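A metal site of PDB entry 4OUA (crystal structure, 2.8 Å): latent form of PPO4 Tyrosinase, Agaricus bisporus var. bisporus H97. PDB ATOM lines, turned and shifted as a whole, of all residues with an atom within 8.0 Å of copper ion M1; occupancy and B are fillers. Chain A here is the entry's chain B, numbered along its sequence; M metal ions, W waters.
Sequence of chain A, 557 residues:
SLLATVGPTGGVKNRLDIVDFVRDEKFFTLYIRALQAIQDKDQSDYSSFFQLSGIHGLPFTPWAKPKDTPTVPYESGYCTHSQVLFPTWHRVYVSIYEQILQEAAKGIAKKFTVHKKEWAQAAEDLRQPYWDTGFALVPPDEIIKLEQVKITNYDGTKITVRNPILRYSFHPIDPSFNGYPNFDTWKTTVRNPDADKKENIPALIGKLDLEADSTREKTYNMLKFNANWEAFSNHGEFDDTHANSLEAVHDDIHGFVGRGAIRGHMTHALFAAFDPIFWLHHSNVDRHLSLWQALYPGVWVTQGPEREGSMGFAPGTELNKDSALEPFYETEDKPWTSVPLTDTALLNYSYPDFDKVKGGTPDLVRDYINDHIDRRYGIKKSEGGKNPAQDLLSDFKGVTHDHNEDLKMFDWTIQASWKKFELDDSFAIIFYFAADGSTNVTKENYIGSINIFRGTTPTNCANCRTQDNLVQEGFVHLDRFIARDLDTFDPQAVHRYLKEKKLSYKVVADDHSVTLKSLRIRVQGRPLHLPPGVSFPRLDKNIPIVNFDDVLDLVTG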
ATOM      1  N   ILE A  55     -12.262  23.925  23.177  1.00  0.00           N
ATOM      2  CA  ILE A  55     -12.127  24.706  21.942  1.00  0.00           C
ATOM      3  C   ILE A  55     -13.443  24.776  21.177  1.00  0.00           C
ATOM      4  O   ILE A  55     -13.804  25.829  20.650  1.00  0.00           O
ATOM      5  CB  ILE A  55     -11.044  24.110  21.029  1.00  0.00           C
ATOM      6  CG1 ILE A  55      -9.673  24.225  21.683  1.00  0.00           C
ATOM      7  CG2 ILE A  55     -11.059  24.806  19.670  1.00  0.00           C
ATOM      8  CD1 ILE A  55      -8.539  23.654  20.857  1.00  0.00           C
ATOM      9  N   HIS A  56     -14.146  23.646  21.112  1.00  0.00           N
ATOM     10  CA  HIS A  56     -15.390  23.547  20.353  1.00  0.00           C
ATOM     11  C   HIS A  56     -16.403  24.603  20.779  1.00  0.00           C
ATOM     12  O   HIS A  56     -16.685  25.547  20.045  1.00  0.00           O
ATOM     13  CB  HIS A  56     -15.991  22.152  20.506  1.00  0.00           C
ATOM     14  CG  HIS A  56     -16.975  21.798  19.436  1.00  0.00           C
ATOM     15  ND1 HIS A  56     -18.338  21.726  19.669  1.00  0.00           N
ATOM     16  CD2 HIS A  56     -16.807  21.497  18.125  1.00  0.00           C
ATOM     17  CE1 HIS A  56     -18.961  21.390  18.559  1.00  0.00           C
ATOM     18  NE2 HIS A  56     -18.050  21.246  17.602  1.00  0.00           N
ATOM     19  N   GLY A  57     -16.950  24.438  21.979  1.00  0.00           N
ATOM     20  CA  GLY A  57     -17.915  25.382  22.515  1.00  0.00           C
ATOM     21  C   GLY A  57     -17.372  26.092  23.743  1.00  0.00           C
ATOM     22  O   GLY A  57     -16.465  26.921  23.640  1.00  0.00           O
ATOM     23  N   TYR A  78     -15.141  28.081  19.116  1.00  0.00           N
ATOM     24  CA  TYR A  78     -14.272  28.162  17.936  1.00  0.00           C
ATOM     25  C   TYR A  78     -14.872  27.429  16.745  1.00  0.00           C
ATOM     26  O   TYR A  78     -14.628  27.807  15.596  1.00  0.00           O
ATOM     27  CB  TYR A  78     -12.897  27.572  18.231  1.00  0.00           C
ATOM     28  CG  TYR A  78     -11.877  28.536  18.794  1.00  0.00           C
ATOM     29  CD1 TYR A  78     -11.299  29.510  17.985  1.00  0.00           C
ATOM     30  CD2 TYR A  78     -11.463  28.454  20.114  1.00  0.00           C
ATOM     31  CE1 TYR A  78     -10.360  30.390  18.495  1.00  0.00           C
ATOM     32  CE2 TYR A  78     -10.526  29.321  20.630  1.00  0.00           C
ATOM     33  CZ  TYR A  78      -9.979  30.289  19.819  1.00  0.00           C
ATOM     34  OH  TYR A  78      -9.037  31.151  20.324  1.00  0.00           O
ATOM     35  N   CYS A  79     -15.649  26.379  17.015  1.00  0.00           N
ATOM     36  CA  CYS A  79     -16.153  25.515  15.956  1.00  0.00           C
ATOM     37  C   CYS A  79     -17.037  26.273  14.978  1.00  0.00           C
ATOM     38  O   CYS A  79     -17.793  27.162  15.378  1.00  0.00           O
ATOM     39  CB  CYS A  79     -16.912  24.320  16.552  1.00  0.00           C
ATOM     40  SG  CYS A  79     -18.535  24.718  17.227  1.00  0.00           S
ATOM     41  N   THR A  80     -16.934  25.917  13.701  1.00  0.00           N
ATOM     42  CA  THR A  80     -17.699  26.569  12.657  1.00  0.00           C
ATOM     43  C   THR A  80     -18.831  25.676  12.171  1.00  0.00           C
ATOM     44  O   THR A  80     -18.597  24.626  11.591  1.00  0.00           O
ATOM     45  CB  THR A  80     -16.807  26.940  11.453  1.00  0.00           C
ATOM     46  OG1 THR A  80     -16.331  25.749  10.828  1.00  0.00           O
ATOM     47  CG2 THR A  80     -15.619  27.778  11.915  1.00  0.00           C
ATOM     48  N   HIS A  81     -20.060  26.104  12.426  1.00  0.00           N
ATOM     49  CA  HIS A  81     -21.224  25.325  12.030  1.00  0.00           C
ATOM     50  C   HIS A  81     -22.175  26.143  11.154  1.00  0.00           C
ATOM     51  O   HIS A  81     -22.265  27.362  11.297  1.00  0.00           O
ATOM     52  CB  HIS A  81     -21.953  24.799  13.280  1.00  0.00           C
ATOM     53  CG  HIS A  81     -21.047  24.138  14.271  1.00  0.00           C
ATOM     54  ND1 HIS A  81     -20.417  24.827  15.284  1.00  0.00           N
ATOM     55  CD2 HIS A  81     -20.660  22.847  14.393  1.00  0.00           C
ATOM     56  CE1 HIS A  81     -19.677  23.981  15.990  1.00  0.00           C
ATOM     57  NE2 HIS A  81     -19.814  22.777  15.470  1.00  0.00           N
ATOM     58  N   PHE A  86     -17.077  24.414   7.757  1.00  0.00           N
ATOM     59  CA  PHE A  86     -17.409  23.300   8.648  1.00  0.00           C
ATOM     60  C   PHE A  86     -16.516  22.075   8.440  1.00  0.00           C
ATOM     61  O   PHE A  86     -15.900  21.604   9.398  1.00  0.00           O
ATOM     62  CB  PHE A  86     -18.881  22.891   8.478  1.00  0.00           C
ATOM     63  CG  PHE A  86     -19.238  21.632   9.211  1.00  0.00           C
ATOM     64  CD1 PHE A  86     -19.538  21.666  10.571  1.00  0.00           C
ATOM     65  CD2 PHE A  86     -19.295  20.416   8.546  1.00  0.00           C
ATOM     66  CE1 PHE A  86     -19.868  20.505  11.250  1.00  0.00           C
ATOM     67  CE2 PHE A  86     -19.625  19.254   9.225  1.00  0.00           C
ATOM     68  CZ  PHE A  86     -19.911  19.305  10.574  1.00  0.00           C
ATOM     69  N   TRP A  89     -12.498  23.039   9.038  1.00  0.00           N
ATOM     70  CA  TRP A  89     -12.164  23.451  10.400  1.00  0.00           C
ATOM     71  C   TRP A  89     -12.094  22.244  11.326  1.00  0.00           C
ATOM     72  O   TRP A  89     -11.194  22.145  12.162  1.00  0.00           O
ATOM     73  CB  TRP A  89     -13.184  24.461  10.931  1.00  0.00           C
ATOM     74  CG  TRP A  89     -12.839  24.934  12.310  1.00  0.00           C
ATOM     75  CD1 TRP A  89     -12.137  26.061  12.647  1.00  0.00           C
ATOM     76  CD2 TRP A  89     -13.167  24.286  13.548  1.00  0.00           C
ATOM     77  NE1 TRP A  89     -12.020  26.154  14.006  1.00  0.00           N
ATOM     78  CE2 TRP A  89     -12.639  25.077  14.586  1.00  0.00           C
ATOM     79  CE3 TRP A  89     -13.852  23.118  13.874  1.00  0.00           C
ATOM     80  CZ2 TRP A  89     -12.778  24.732  15.925  1.00  0.00           C
ATOM     81  CZ3 TRP A  89     -13.990  22.774  15.213  1.00  0.00           C
ATOM     82  CH2 TRP A  89     -13.449  23.578  16.216  1.00  0.00           C
ATOM     83  N   HIS A  90     -13.065  21.341  11.194  1.00  0.00           N
ATOM     84  CA  HIS A  90     -13.101  20.153  12.030  1.00  0.00           C
ATOM     85  C   HIS A  90     -11.994  19.175  11.682  1.00  0.00           C
ATOM     86  O   HIS A  90     -11.545  18.406  12.537  1.00  0.00           O
ATOM     87  CB  HIS A  90     -14.469  19.468  11.915  1.00  0.00           C
ATOM     88  CG  HIS A  90     -15.571  20.217  12.607  1.00  0.00           C
ATOM     89  ND1 HIS A  90     -16.170  21.334  12.073  1.00  0.00           N
ATOM     90  CD2 HIS A  90     -16.185  20.001  13.795  1.00  0.00           C
ATOM     91  CE1 HIS A  90     -17.101  21.773  12.900  1.00  0.00           C
ATOM     92  NE2 HIS A  90     -17.129  20.976  13.953  1.00  0.00           N
ATOM     93  N   TYR A  93      -9.155  20.170  13.491  1.00  0.00           N
ATOM     94  CA  TYR A  93      -9.554  20.036  14.883  1.00  0.00           C
ATOM     95  C   TYR A  93      -9.305  18.626  15.419  1.00  0.00           C
ATOM     96  O   TYR A  93      -8.936  18.450  16.572  1.00  0.00           O
ATOM     97  CB  TYR A  93     -11.029  20.389  15.061  1.00  0.00           C
ATOM     98  CG  TYR A  93     -11.500  20.408  16.499  1.00  0.00           C
ATOM     99  CD1 TYR A  93     -10.671  20.869  17.508  1.00  0.00           C
ATOM    100  CD2 TYR A  93     -12.775  19.977  16.838  1.00  0.00           C
ATOM    101  CE1 TYR A  93     -11.095  20.893  18.829  1.00  0.00           C
ATOM    102  CE2 TYR A  93     -13.208  19.999  18.155  1.00  0.00           C
ATOM    103  CZ  TYR A  93     -12.362  20.459  19.148  1.00  0.00           C
ATOM    104  OH  TYR A  93     -12.790  20.476  20.453  1.00  0.00           O
ATOM    105  N   GLU A 247     -22.853  17.957   7.195  1.00  0.00           N
ATOM    106  CA  GLU A 247     -23.202  18.429   8.529  1.00  0.00           C
ATOM    107  C   GLU A 247     -24.539  17.850   8.991  1.00  0.00           C
ATOM    108  O   GLU A 247     -24.711  17.530  10.168  1.00  0.00           O
ATOM    109  CB  GLU A 247     -23.244  19.950   8.560  1.00  0.00           C
ATOM    110  CG  GLU A 247     -23.292  20.555   9.957  1.00  0.00           C
ATOM    111  CD  GLU A 247     -23.310  22.079   9.929  1.00  0.00           C
ATOM    112  OE1 GLU A 247     -23.721  22.644   8.904  1.00  0.00           O
ATOM    113  OE2 GLU A 247     -22.912  22.693  10.940  1.00  0.00           O
ATOM    114  N   HIS A 250     -24.120  14.503   9.995  1.00  0.00           N
ATOM    115  CA  HIS A 250     -23.261  14.674  11.163  1.00  0.00           C
ATOM    116  C   HIS A 250     -24.068  14.973  12.426  1.00  0.00           C
ATOM    117  O   HIS A 250     -23.765  14.458  13.498  1.00  0.00           O
ATOM    118  CB  HIS A 250     -22.262  15.799  10.892  1.00  0.00           C
ATOM    119  CG  HIS A 250     -21.766  16.473  12.135  1.00  0.00           C
ATOM    120  ND1 HIS A 250     -22.328  17.625  12.632  1.00  0.00           N
ATOM    121  CD2 HIS A 250     -20.746  16.161  12.976  1.00  0.00           C
ATOM    122  CE1 HIS A 250     -21.689  17.991  13.726  1.00  0.00           C
ATOM    123  NE2 HIS A 250     -20.721  17.121  13.949  1.00  0.00           N
ATOM    124  N   ASP A 251     -25.100  15.803  12.288  1.00  0.00           N
ATOM    125  CA  ASP A 251     -25.908  16.205  13.432  1.00  0.00           C
ATOM    126  C   ASP A 251     -26.712  15.042  14.000  1.00  0.00           C
ATOM    127  O   ASP A 251     -27.015  15.002  15.192  1.00  0.00           O
ATOM    128  CB  ASP A 251     -26.851  17.345  13.051  1.00  0.00           C
ATOM    129  CG  ASP A 251     -26.120  18.569  12.548  1.00  0.00           C
ATOM    130  OD1 ASP A 251     -26.714  19.331  11.760  1.00  0.00           O
ATOM    131  OD2 ASP A 251     -24.944  18.770  12.923  1.00  0.00           O
ATOM    132  N   HIS A 254     -25.043  13.273  16.810  1.00  0.00           N
ATOM    133  CA  HIS A 254     -25.041  14.086  18.024  1.00  0.00           C
ATOM    134  C   HIS A 254     -26.359  13.952  18.774  1.00  0.00           C
ATOM    135  O   HIS A 254     -26.386  13.911  20.002  1.00  0.00           O
ATOM    136  CB  HIS A 254     -24.781  15.550  17.689  1.00  0.00           C
ATOM    137  CG  HIS A 254     -23.352  15.848  17.389  1.00  0.00           C
ATOM    138  ND1 HIS A 254     -22.410  16.051  18.372  1.00  0.00           N
ATOM    139  CD2 HIS A 254     -22.694  15.994  16.213  1.00  0.00           C
ATOM    140  CE1 HIS A 254     -21.232  16.297  17.820  1.00  0.00           C
ATOM    141  NE2 HIS A 254     -21.383  16.268  16.508  1.00  0.00           N
ATOM    142  N   ALA A 269     -23.929  21.782  21.381  1.00  0.00           N
ATOM    143  CA  ALA A 269     -22.677  22.171  20.730  1.00  0.00           C
ATOM    144  C   ALA A 269     -21.662  22.795  21.681  1.00  0.00           C
ATOM    145  O   ALA A 269     -20.467  22.842  21.386  1.00  0.00           O
ATOM    146  CB  ALA A 269     -22.954  23.123  19.579  1.00  0.00           C
ATOM    147  N   ALA A 272     -20.679  19.208  23.657  1.00  0.00           N
ATOM    148  CA  ALA A 272     -20.582  17.952  22.909  1.00  0.00           C
ATOM    149  C   ALA A 272     -19.164  17.398  22.823  1.00  0.00           C
ATOM    150  O   ALA A 272     -18.968  16.184  22.791  1.00  0.00           O
ATOM    151  CB  ALA A 272     -21.151  18.140  21.503  1.00  0.00           C
ATOM    152  N   ALA A 273     -18.168  18.285  22.788  1.00  0.00           N
ATOM    153  CA  ALA A 273     -16.784  17.862  22.605  1.00  0.00           C
ATOM    154  C   ALA A 273     -16.227  17.169  23.851  1.00  0.00           C
ATOM    155  O   ALA A 273     -15.226  16.466  23.777  1.00  0.00           O
ATOM    156  CB  ALA A 273     -15.921  19.059  22.232  1.00  0.00           C
ATOM    157  N   PHE A 278     -17.048  11.873  21.011  1.00  0.00           N
ATOM    158  CA  PHE A 278     -17.070  12.979  20.063  1.00  0.00           C
ATOM    159  C   PHE A 278     -16.051  12.800  18.951  1.00  0.00           C
ATOM    160  O   PHE A 278     -16.349  13.006  17.780  1.00  0.00           O
ATOM    161  CB  PHE A 278     -16.826  14.289  20.814  1.00  0.00           C
ATOM    162  CG  PHE A 278     -16.820  15.517  19.936  1.00  0.00           C
ATOM    163  CD1 PHE A 278     -15.656  15.947  19.337  1.00  0.00           C
ATOM    164  CD2 PHE A 278     -17.980  16.250  19.756  1.00  0.00           C
ATOM    165  CE1 PHE A 278     -15.647  17.082  18.549  1.00  0.00           C
ATOM    166  CE2 PHE A 278     -17.981  17.384  18.965  1.00  0.00           C
ATOM    167  CZ  PHE A 278     -16.806  17.805  18.366  1.00  0.00           C
ATOM    168  N   HIS A 282     -16.154  12.404  14.752  1.00  0.00           N
ATOM    169  CA  HIS A 282     -15.592  13.346  13.799  1.00  0.00           C
ATOM    170  C   HIS A 282     -14.439  12.757  13.007  1.00  0.00           C
ATOM    171  O   HIS A 282     -14.074  13.259  11.941  1.00  0.00           O
ATOM    172  CB  HIS A 282     -15.147  14.623  14.509  1.00  0.00           C
ATOM    173  CG  HIS A 282     -16.268  15.565  14.792  1.00  0.00           C
ATOM    174  ND1 HIS A 282     -16.736  16.464  13.856  1.00  0.00           N
ATOM    175  CD2 HIS A 282     -17.026  15.743  15.900  1.00  0.00           C
ATOM    176  CE1 HIS A 282     -17.735  17.159  14.383  1.00  0.00           C
ATOM    177  NE2 HIS A 282     -17.924  16.742  15.617  1.00  0.00           N
ATOM    178  N   GLU A 308     -24.152  31.899  12.369  1.00  0.00           N
ATOM    179  CA  GLU A 308     -24.447  31.797  13.791  1.00  0.00           C
ATOM    180  C   GLU A 308     -23.377  32.460  14.652  1.00  0.00           C
ATOM    181  O   GLU A 308     -23.666  32.932  15.757  1.00  0.00           O
ATOM    182  CB  GLU A 308     -24.620  30.335  14.204  1.00  0.00           C
ATOM    183  CG  GLU A 308     -23.352  29.501  14.134  1.00  0.00           C
ATOM    184  CD  GLU A 308     -23.594  28.054  14.527  1.00  0.00           C
ATOM    185  OE1 GLU A 308     -24.767  27.606  14.454  1.00  0.00           O
ATOM    186  OE2 GLU A 308     -22.619  27.364  14.894  1.00  0.00           O
ATOM    187  N   PHE A 453     -28.705  19.973  15.838  1.00  0.00           N
ATOM    188  CA  PHE A 453     -27.552  20.182  16.698  1.00  0.00           C
ATOM    189  C   PHE A 453     -27.308  21.676  16.883  1.00  0.00           C
ATOM    190  O   PHE A 453     -26.765  22.337  15.994  1.00  0.00           O
ATOM    191  CB  PHE A 453     -26.312  19.501  16.108  1.00  0.00           C
ATOM    192  CG  PHE A 453     -25.128  19.515  17.028  1.00  0.00           C
ATOM    193  CD1 PHE A 453     -25.250  19.133  18.358  1.00  0.00           C
ATOM    194  CD2 PHE A 453     -23.869  19.880  16.552  1.00  0.00           C
ATOM    195  CE1 PHE A 453     -24.154  19.133  19.204  1.00  0.00           C
ATOM    196  CE2 PHE A 453     -22.773  19.880  17.399  1.00  0.00           C
ATOM    197  CZ  PHE A 453     -22.912  19.510  18.716  1.00  0.00           C
HETATM  198 CU    CU M   1     -18.173  21.553  15.602  1.00  0.00          CU
HETATM  199 CU    CU M   2     -19.837  17.193  15.794  1.00  0.00          CU
HETATM  200  O   HOH W   1     -19.011  19.373  15.661  1.00  0.00           O
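A ring nitrogen (ND1) of His 81 sits close to the side-chain carboxylate (OE2) of Glu 308 (3.4 Å). The backbone carbonyl oxygen (O) of His 56 is in hydrogen-bond range of the backbone NH (N) of Tyr 78 (3.1 Å). A ring nitrogen (ND1) of His 56 sits at hydrogen-bond distance from the backbone carbonyl oxygen (O) of Ala 269 (3.0 Å). ND1 of His 90 sits at hydrogen-bond distance from O of Phe 86 (2.7 Å). CE1 of His 81 is bonded to SG of Cys 79. The backbone carbonyl oxygen (O) of His 56 is in hydrogen-bond range of the backbone NH (N) of Cys 79, 3.3 Å away.
Merely in contact with copper ion M1: Cys 79 (3.2 Å).
Copper ion M1 is bound by NE2 of His 56 (2.0 Å), NE2 of His 90 (2.0 Å), NE2 of His 81 (2.1 Å) and water W1 (2.3 Å).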
